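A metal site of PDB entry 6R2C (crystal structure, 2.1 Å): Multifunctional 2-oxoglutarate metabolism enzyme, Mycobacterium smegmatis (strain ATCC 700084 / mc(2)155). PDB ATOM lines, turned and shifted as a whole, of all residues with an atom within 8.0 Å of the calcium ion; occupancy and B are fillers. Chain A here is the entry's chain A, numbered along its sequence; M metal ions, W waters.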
ATOM      1  N   LYS A 535     -20.006  28.011   7.786  1.00  0.00           N
ATOM      2  CA  LYS A 535     -19.633  27.585   6.439  1.00  0.00           C
ATOM      3  C   LYS A 535     -18.184  27.910   6.095  1.00  0.00           C
ATOM      4  O   LYS A 535     -17.688  28.980   6.431  1.00  0.00           O
ATOM      5  CB  LYS A 535     -20.561  28.219   5.394  1.00  0.00           C
ATOM      6  CG  LYS A 535     -20.680  27.395   4.119  1.00  0.00           C
ATOM      7  CD  LYS A 535     -21.695  27.957   3.149  1.00  0.00           C
ATOM      8  CE  LYS A 535     -21.885  27.051   1.964  1.00  0.00           C
ATOM      9  NZ  LYS A 535     -22.593  25.789   2.327  1.00  0.00           N
ATOM     10  N   PRO A 608     -18.733  19.448  -0.936  1.00  0.00           N
ATOM     11  CA  PRO A 608     -20.026  20.060  -1.342  1.00  0.00           C
ATOM     12  C   PRO A 608     -20.577  21.079  -0.346  1.00  0.00           C
ATOM     13  O   PRO A 608     -21.440  21.881  -0.718  1.00  0.00           O
ATOM     14  CB  PRO A 608     -20.969  18.858  -1.453  1.00  0.00           C
ATOM     15  CG  PRO A 608     -20.074  17.649  -1.506  1.00  0.00           C
ATOM     16  CD  PRO A 608     -18.889  17.999  -0.684  1.00  0.00           C
ATOM     17  N   ALA A 610     -18.766  23.404   1.115  1.00  0.00           N
ATOM     18  CA  ALA A 610     -17.972  24.628   0.990  1.00  0.00           C
ATOM     19  C   ALA A 610     -18.619  25.635   0.022  1.00  0.00           C
ATOM     20  O   ALA A 610     -19.285  25.238  -0.927  1.00  0.00           O
ATOM     21  CB  ALA A 610     -16.571  24.292   0.505  1.00  0.00           C
ATOM     22  N   MET A 611     -18.399  26.932   0.292  1.00  0.00           N
ATOM     23  CA  MET A 611     -18.801  28.040  -0.574  1.00  0.00           C
ATOM     24  C   MET A 611     -17.544  28.341  -1.398  1.00  0.00           C
ATOM     25  O   MET A 611     -16.560  28.790  -0.832  1.00  0.00           O
ATOM     26  CB  MET A 611     -19.295  29.234   0.271  1.00  0.00           C
ATOM     27  CG  MET A 611     -19.715  30.455  -0.545  1.00  0.00           C
ATOM     28  SD  MET A 611     -21.392  30.350  -1.232  1.00  0.00           S
ATOM     29  CE  MET A 611     -21.509  31.933  -1.998  1.00  0.00           C
ATOM     30  N   SER A 644     -21.588  20.098  -8.613  1.00  0.00           N
ATOM     31  CA  SER A 644     -20.700  21.196  -8.250  1.00  0.00           C
ATOM     32  C   SER A 644     -21.512  22.426  -7.874  1.00  0.00           C
ATOM     33  O   SER A 644     -22.478  22.745  -8.554  1.00  0.00           O
ATOM     34  CB  SER A 644     -19.782  21.532  -9.425  1.00  0.00           C
ATOM     35  OG  SER A 644     -18.928  22.624  -9.127  1.00  0.00           O
ATOM     36  N   ASP A 645     -21.093  23.122  -6.813  1.00  0.00           N
ATOM     37  CA  ASP A 645     -21.727  24.375  -6.381  1.00  0.00           C
ATOM     38  C   ASP A 645     -20.770  25.554  -6.620  1.00  0.00           C
ATOM     39  O   ASP A 645     -20.935  26.599  -5.999  1.00  0.00           O
ATOM     40  CB  ASP A 645     -22.160  24.291  -4.898  1.00  0.00           C
ATOM     41  CG  ASP A 645     -23.454  24.995  -4.553  1.00  0.00           C
ATOM     42  OD1 ASP A 645     -24.368  25.046  -5.411  1.00  0.00           O
ATOM     43  OD2 ASP A 645     -23.601  25.457  -3.404  1.00  0.00           O
ATOM     44  N   VAL A 646     -19.798  25.403  -7.542  1.00  0.00           N
ATOM     45  CA  VAL A 646     -18.796  26.439  -7.846  1.00  0.00           C
ATOM     46  C   VAL A 646     -19.467  27.748  -8.344  1.00  0.00           C
ATOM     47  O   VAL A 646     -20.471  27.717  -9.045  1.00  0.00           O
ATOM     48  CB  VAL A 646     -17.674  25.938  -8.799  1.00  0.00           C
ATOM     49  CG1 VAL A 646     -18.155  25.758 -10.252  1.00  0.00           C
ATOM     50  CG2 VAL A 646     -16.430  26.834  -8.740  1.00  0.00           C
ATOM     51  N   VAL A 647     -18.925  28.894  -7.906  1.00  0.00           N
ATOM     52  CA  VAL A 647     -19.361  30.229  -8.308  1.00  0.00           C
ATOM     53  C   VAL A 647     -18.289  30.848  -9.202  1.00  0.00           C
ATOM     54  O   VAL A 647     -17.123  30.853  -8.822  1.00  0.00           O
ATOM     55  CB  VAL A 647     -19.688  31.174  -7.110  1.00  0.00           C
ATOM     56  CG1 VAL A 647     -20.266  32.501  -7.585  1.00  0.00           C
ATOM     57  CG2 VAL A 647     -20.612  30.506  -6.105  1.00  0.00           C
ATOM     58  N   THR A 679     -27.217  28.378 -12.627  1.00  0.00           N
ATOM     59  CA  THR A 679     -27.912  29.616 -12.278  1.00  0.00           C
ATOM     60  C   THR A 679     -27.057  30.736 -12.868  1.00  0.00           C
ATOM     61  O   THR A 679     -25.832  30.742 -12.680  1.00  0.00           O
ATOM     62  CB  THR A 679     -28.163  29.753 -10.769  1.00  0.00           C
ATOM     63  OG1 THR A 679     -28.821  28.571 -10.291  1.00  0.00           O
ATOM     64  CG2 THR A 679     -29.016  30.971 -10.421  1.00  0.00           C
ATOM     65  N   LEU A 692     -28.309  36.724  -3.271  1.00  0.00           N
ATOM     66  CA  LEU A 692     -27.975  35.748  -4.305  1.00  0.00           C
ATOM     67  C   LEU A 692     -26.888  34.782  -3.798  1.00  0.00           C
ATOM     68  O   LEU A 692     -27.000  33.577  -3.993  1.00  0.00           O
ATOM     69  CB  LEU A 692     -27.515  36.467  -5.594  1.00  0.00           C
ATOM     70  CG  LEU A 692     -27.044  35.568  -6.770  1.00  0.00           C
ATOM     71  CD1 LEU A 692     -28.227  35.039  -7.576  1.00  0.00           C
ATOM     72  CD2 LEU A 692     -26.058  36.289  -7.657  1.00  0.00           C
ATOM     73  N   LEU A 693     -25.838  35.326  -3.128  1.00  0.00           N
ATOM     74  CA  LEU A 693     -24.731  34.528  -2.578  1.00  0.00           C
ATOM     75  C   LEU A 693     -25.189  33.688  -1.386  1.00  0.00           C
ATOM     76  O   LEU A 693     -24.783  32.538  -1.255  1.00  0.00           O
ATOM     77  CB  LEU A 693     -23.543  35.418  -2.170  1.00  0.00           C
ATOM     78  CG  LEU A 693     -22.748  36.112  -3.295  1.00  0.00           C
ATOM     79  CD1 LEU A 693     -21.626  36.935  -2.719  1.00  0.00           C
ATOM     80  CD2 LEU A 693     -22.156  35.090  -4.296  1.00  0.00           C
ATOM     81  N   ARG A 694     -26.034  34.270  -0.513  1.00  0.00           N
ATOM     82  CA  ARG A 694     -26.550  33.547   0.648  1.00  0.00           C
ATOM     83  C   ARG A 694     -27.521  32.446   0.229  1.00  0.00           C
ATOM     84  O   ARG A 694     -27.425  31.349   0.777  1.00  0.00           O
ATOM     85  CB  ARG A 694     -27.169  34.487   1.683  1.00  0.00           C
ATOM     86  CG  ARG A 694     -26.069  35.157   2.508  1.00  0.00           C
ATOM     87  CD  ARG A 694     -26.569  35.994   3.658  1.00  0.00           C
ATOM     88  NE  ARG A 694     -27.484  35.287   4.563  1.00  0.00           N
ATOM     89  CZ  ARG A 694     -27.111  34.443   5.523  1.00  0.00           C
ATOM     90  NH1 ARG A 694     -25.831  34.163   5.716  1.00  0.00           N
ATOM     91  NH2 ARG A 694     -28.027  33.877   6.293  1.00  0.00           N
ATOM     92  N   ARG A 695     -28.392  32.698  -0.783  1.00  0.00           N
ATOM     93  CA  ARG A 695     -29.318  31.679  -1.305  1.00  0.00           C
ATOM     94  C   ARG A 695     -28.505  30.516  -1.850  1.00  0.00           C
ATOM     95  O   ARG A 695     -28.774  29.374  -1.496  1.00  0.00           O
ATOM     96  CB  ARG A 695     -30.268  32.256  -2.388  1.00  0.00           C
ATOM     97  CG  ARG A 695     -31.253  31.225  -2.956  1.00  0.00           C
ATOM     98  CD  ARG A 695     -32.125  31.762  -4.093  1.00  0.00           C
ATOM     99  NE  ARG A 695     -31.355  32.087  -5.292  1.00  0.00           N
ATOM    100  CZ  ARG A 695     -31.875  32.345  -6.483  1.00  0.00           C
ATOM    101  NH1 ARG A 695     -33.181  32.301  -6.662  1.00  0.00           N
ATOM    102  NH2 ARG A 695     -31.084  32.645  -7.510  1.00  0.00           N
ATOM    103  N   HIS A 696     -27.469  30.836  -2.664  1.00  0.00           N
ATOM    104  CA  HIS A 696     -26.583  29.861  -3.284  1.00  0.00           C
ATOM    105  C   HIS A 696     -25.906  28.933  -2.256  1.00  0.00           C
ATOM    106  O   HIS A 696     -25.841  27.733  -2.491  1.00  0.00           O
ATOM    107  CB  HIS A 696     -25.518  30.559  -4.130  1.00  0.00           C
ATOM    108  CG  HIS A 696     -24.634  29.589  -4.843  1.00  0.00           C
ATOM    109  ND1 HIS A 696     -25.096  28.872  -5.937  1.00  0.00           N
ATOM    110  CD2 HIS A 696     -23.381  29.197  -4.560  1.00  0.00           C
ATOM    111  CE1 HIS A 696     -24.080  28.092  -6.295  1.00  0.00           C
ATOM    112  NE2 HIS A 696     -23.035  28.248  -5.498  1.00  0.00           N
ATOM    113  N   GLY A 697     -25.390  29.500  -1.175  1.00  0.00           N
ATOM    114  CA  GLY A 697     -24.717  28.719  -0.144  1.00  0.00           C
ATOM    115  C   GLY A 697     -25.622  27.969   0.818  1.00  0.00           C
ATOM    116  O   GLY A 697     -25.158  27.047   1.489  1.00  0.00           O
ATOM    117  N   LYS A 698     -26.909  28.359   0.913  1.00  0.00           N
ATOM    118  CA  LYS A 698     -27.846  27.778   1.889  1.00  0.00           C
ATOM    119  C   LYS A 698     -29.020  26.965   1.290  1.00  0.00           C
ATOM    120  O   LYS A 698     -29.750  26.353   2.071  1.00  0.00           O
ATOM    121  CB  LYS A 698     -28.430  28.896   2.773  1.00  0.00           C
ATOM    122  CG  LYS A 698     -27.397  29.616   3.652  1.00  0.00           C
ATOM    123  CD  LYS A 698     -27.990  30.876   4.317  1.00  0.00           C
ATOM    124  CE  LYS A 698     -28.879  30.602   5.518  1.00  0.00           C
ATOM    125  NZ  LYS A 698     -28.122  30.014   6.656  1.00  0.00           N
ATOM    126  N   ASP A 699     -29.211  26.963  -0.045  1.00  0.00           N
ATOM    127  CA  ASP A 699     -30.347  26.279  -0.704  1.00  0.00           C
ATOM    128  C   ASP A 699     -30.275  24.725  -0.686  1.00  0.00           C
ATOM    129  O   ASP A 699     -31.257  24.077  -1.029  1.00  0.00           O
ATOM    130  CB  ASP A 699     -30.505  26.764  -2.167  1.00  0.00           C
ATOM    131  CG  ASP A 699     -29.298  26.598  -3.088  1.00  0.00           C
ATOM    132  OD1 ASP A 699     -28.315  25.944  -2.663  1.00  0.00           O
ATOM    133  OD2 ASP A 699     -29.349  27.117  -4.217  1.00  0.00           O
ATOM    134  N   GLY A 700     -29.113  24.175  -0.315  1.00  0.00           N
ATOM    135  CA  GLY A 700     -28.901  22.724  -0.253  1.00  0.00           C
ATOM    136  C   GLY A 700     -28.893  22.037  -1.604  1.00  0.00           C
ATOM    137  O   GLY A 700     -29.058  20.811  -1.682  1.00  0.00           O
ATOM    138  N   ILE A 701     -28.722  22.825  -2.682  1.00  0.00           N
ATOM    139  CA  ILE A 701     -28.697  22.378  -4.081  1.00  0.00           C
ATOM    140  C   ILE A 701     -27.270  22.591  -4.617  1.00  0.00           C
ATOM    141  O   ILE A 701     -26.709  23.661  -4.428  1.00  0.00           O
ATOM    142  CB  ILE A 701     -29.789  23.140  -4.890  1.00  0.00           C
ATOM    143  CG1 ILE A 701     -31.173  22.484  -4.694  1.00  0.00           C
ATOM    144  CG2 ILE A 701     -29.451  23.241  -6.401  1.00  0.00           C
ATOM    145  CD1 ILE A 701     -32.366  23.464  -4.725  1.00  0.00           C
ATOM    146  N   GLN A 702     -26.683  21.554  -5.246  1.00  0.00           N
ATOM    147  CA  GLN A 702     -25.351  21.664  -5.820  1.00  0.00           C
ATOM    148  C   GLN A 702     -25.508  21.984  -7.295  1.00  0.00           C
ATOM    149  O   GLN A 702     -25.842  21.097  -8.109  1.00  0.00           O
ATOM    150  CB  GLN A 702     -24.515  20.394  -5.569  1.00  0.00           C
ATOM    151  CG  GLN A 702     -24.444  19.935  -4.108  1.00  0.00           C
ATOM    152  CD  GLN A 702     -23.863  20.976  -3.185  1.00  0.00           C
ATOM    153  OE1 GLN A 702     -22.681  21.314  -3.261  1.00  0.00           O
ATOM    154  NE2 GLN A 702     -24.688  21.508  -2.289  1.00  0.00           N
ATOM    155  N   ARG A 703     -25.364  23.271  -7.626  1.00  0.00           N
ATOM    156  CA  ARG A 703     -25.544  23.820  -8.968  1.00  0.00           C
ATOM    157  C   ARG A 703     -24.630  25.024  -9.175  1.00  0.00           C
ATOM    158  O   ARG A 703     -24.642  25.922  -8.346  1.00  0.00           O
ATOM    159  CB  ARG A 703     -27.012  24.213  -9.169  1.00  0.00           C
ATOM    160  CG  ARG A 703     -27.400  24.527 -10.609  1.00  0.00           C
ATOM    161  CD  ARG A 703     -28.904  24.626 -10.763  1.00  0.00           C
ATOM    162  NE  ARG A 703     -29.539  23.349 -10.436  1.00  0.00           N
ATOM    163  CZ  ARG A 703     -30.820  23.203 -10.111  1.00  0.00           C
ATOM    164  NH1 ARG A 703     -31.631  24.249 -10.076  1.00  0.00           N
ATOM    165  NH2 ARG A 703     -31.301  22.002  -9.821  1.00  0.00           N
ATOM    166  N   PRO A 704     -23.847  25.090 -10.277  1.00  0.00           N
ATOM    167  CA  PRO A 704     -22.958  26.243 -10.468  1.00  0.00           C
ATOM    168  C   PRO A 704     -23.717  27.557 -10.649  1.00  0.00           C
ATOM    169  O   PRO A 704     -24.821  27.587 -11.179  1.00  0.00           O
ATOM    170  CB  PRO A 704     -22.162  25.887 -11.726  1.00  0.00           C
ATOM    171  CG  PRO A 704     -22.274  24.381 -11.830  1.00  0.00           C
ATOM    172  CD  PRO A 704     -23.659  24.096 -11.364  1.00  0.00           C
ATOM    173  N   LEU A 705     -23.094  28.644 -10.168  1.00  0.00           N
ATOM    174  CA  LEU A 705     -23.629  29.996 -10.252  1.00  0.00           C
ATOM    175  C   LEU A 705     -22.671  30.869 -11.051  1.00  0.00           C
ATOM    176  O   LEU A 705     -21.491  30.952 -10.715  1.00  0.00           O
ATOM    177  CB  LEU A 705     -23.868  30.574  -8.841  1.00  0.00           C
ATOM    178  CG  LEU A 705     -24.271  32.061  -8.724  1.00  0.00           C
ATOM    179  CD1 LEU A 705     -25.647  32.316  -9.336  1.00  0.00           C
ATOM    180  CD2 LEU A 705     -24.241  32.525  -7.287  1.00  0.00           C
HETATM  181 CA    CA M   1     -26.022  25.713  -3.521  1.00  0.00          CA
HETATM  182  O   HOH W   1     -25.389  24.556  -1.451  1.00  0.00           O
HETATM  183  O   HOH W   2     -26.939  26.514  -5.205  1.00  0.00           O
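N of Arg 703 lies close to OD1 of Asp 645, 3.0 Å away.
The calcium ion is bound by water W2 (2.1 Å), the backbone carbonyl oxygen (O) of His 696 (2.3 Å), the backbone carbonyl oxygen (O) of Ile 701 (2.3 Å), the side-chain carboxylate (OD2) of Asp 645 (2.4 Å), water W1 (2.5 Å), the side-chain carboxylate (OD1) of Asp 699 (2.5 Å) and the side-chain carboxylate (OD1) of Asp 645 (2.6 Å).
Water W2 bridges OD2 of Asp 699 (2.7 Å) and ND1 of His 696 (3.1 Å).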
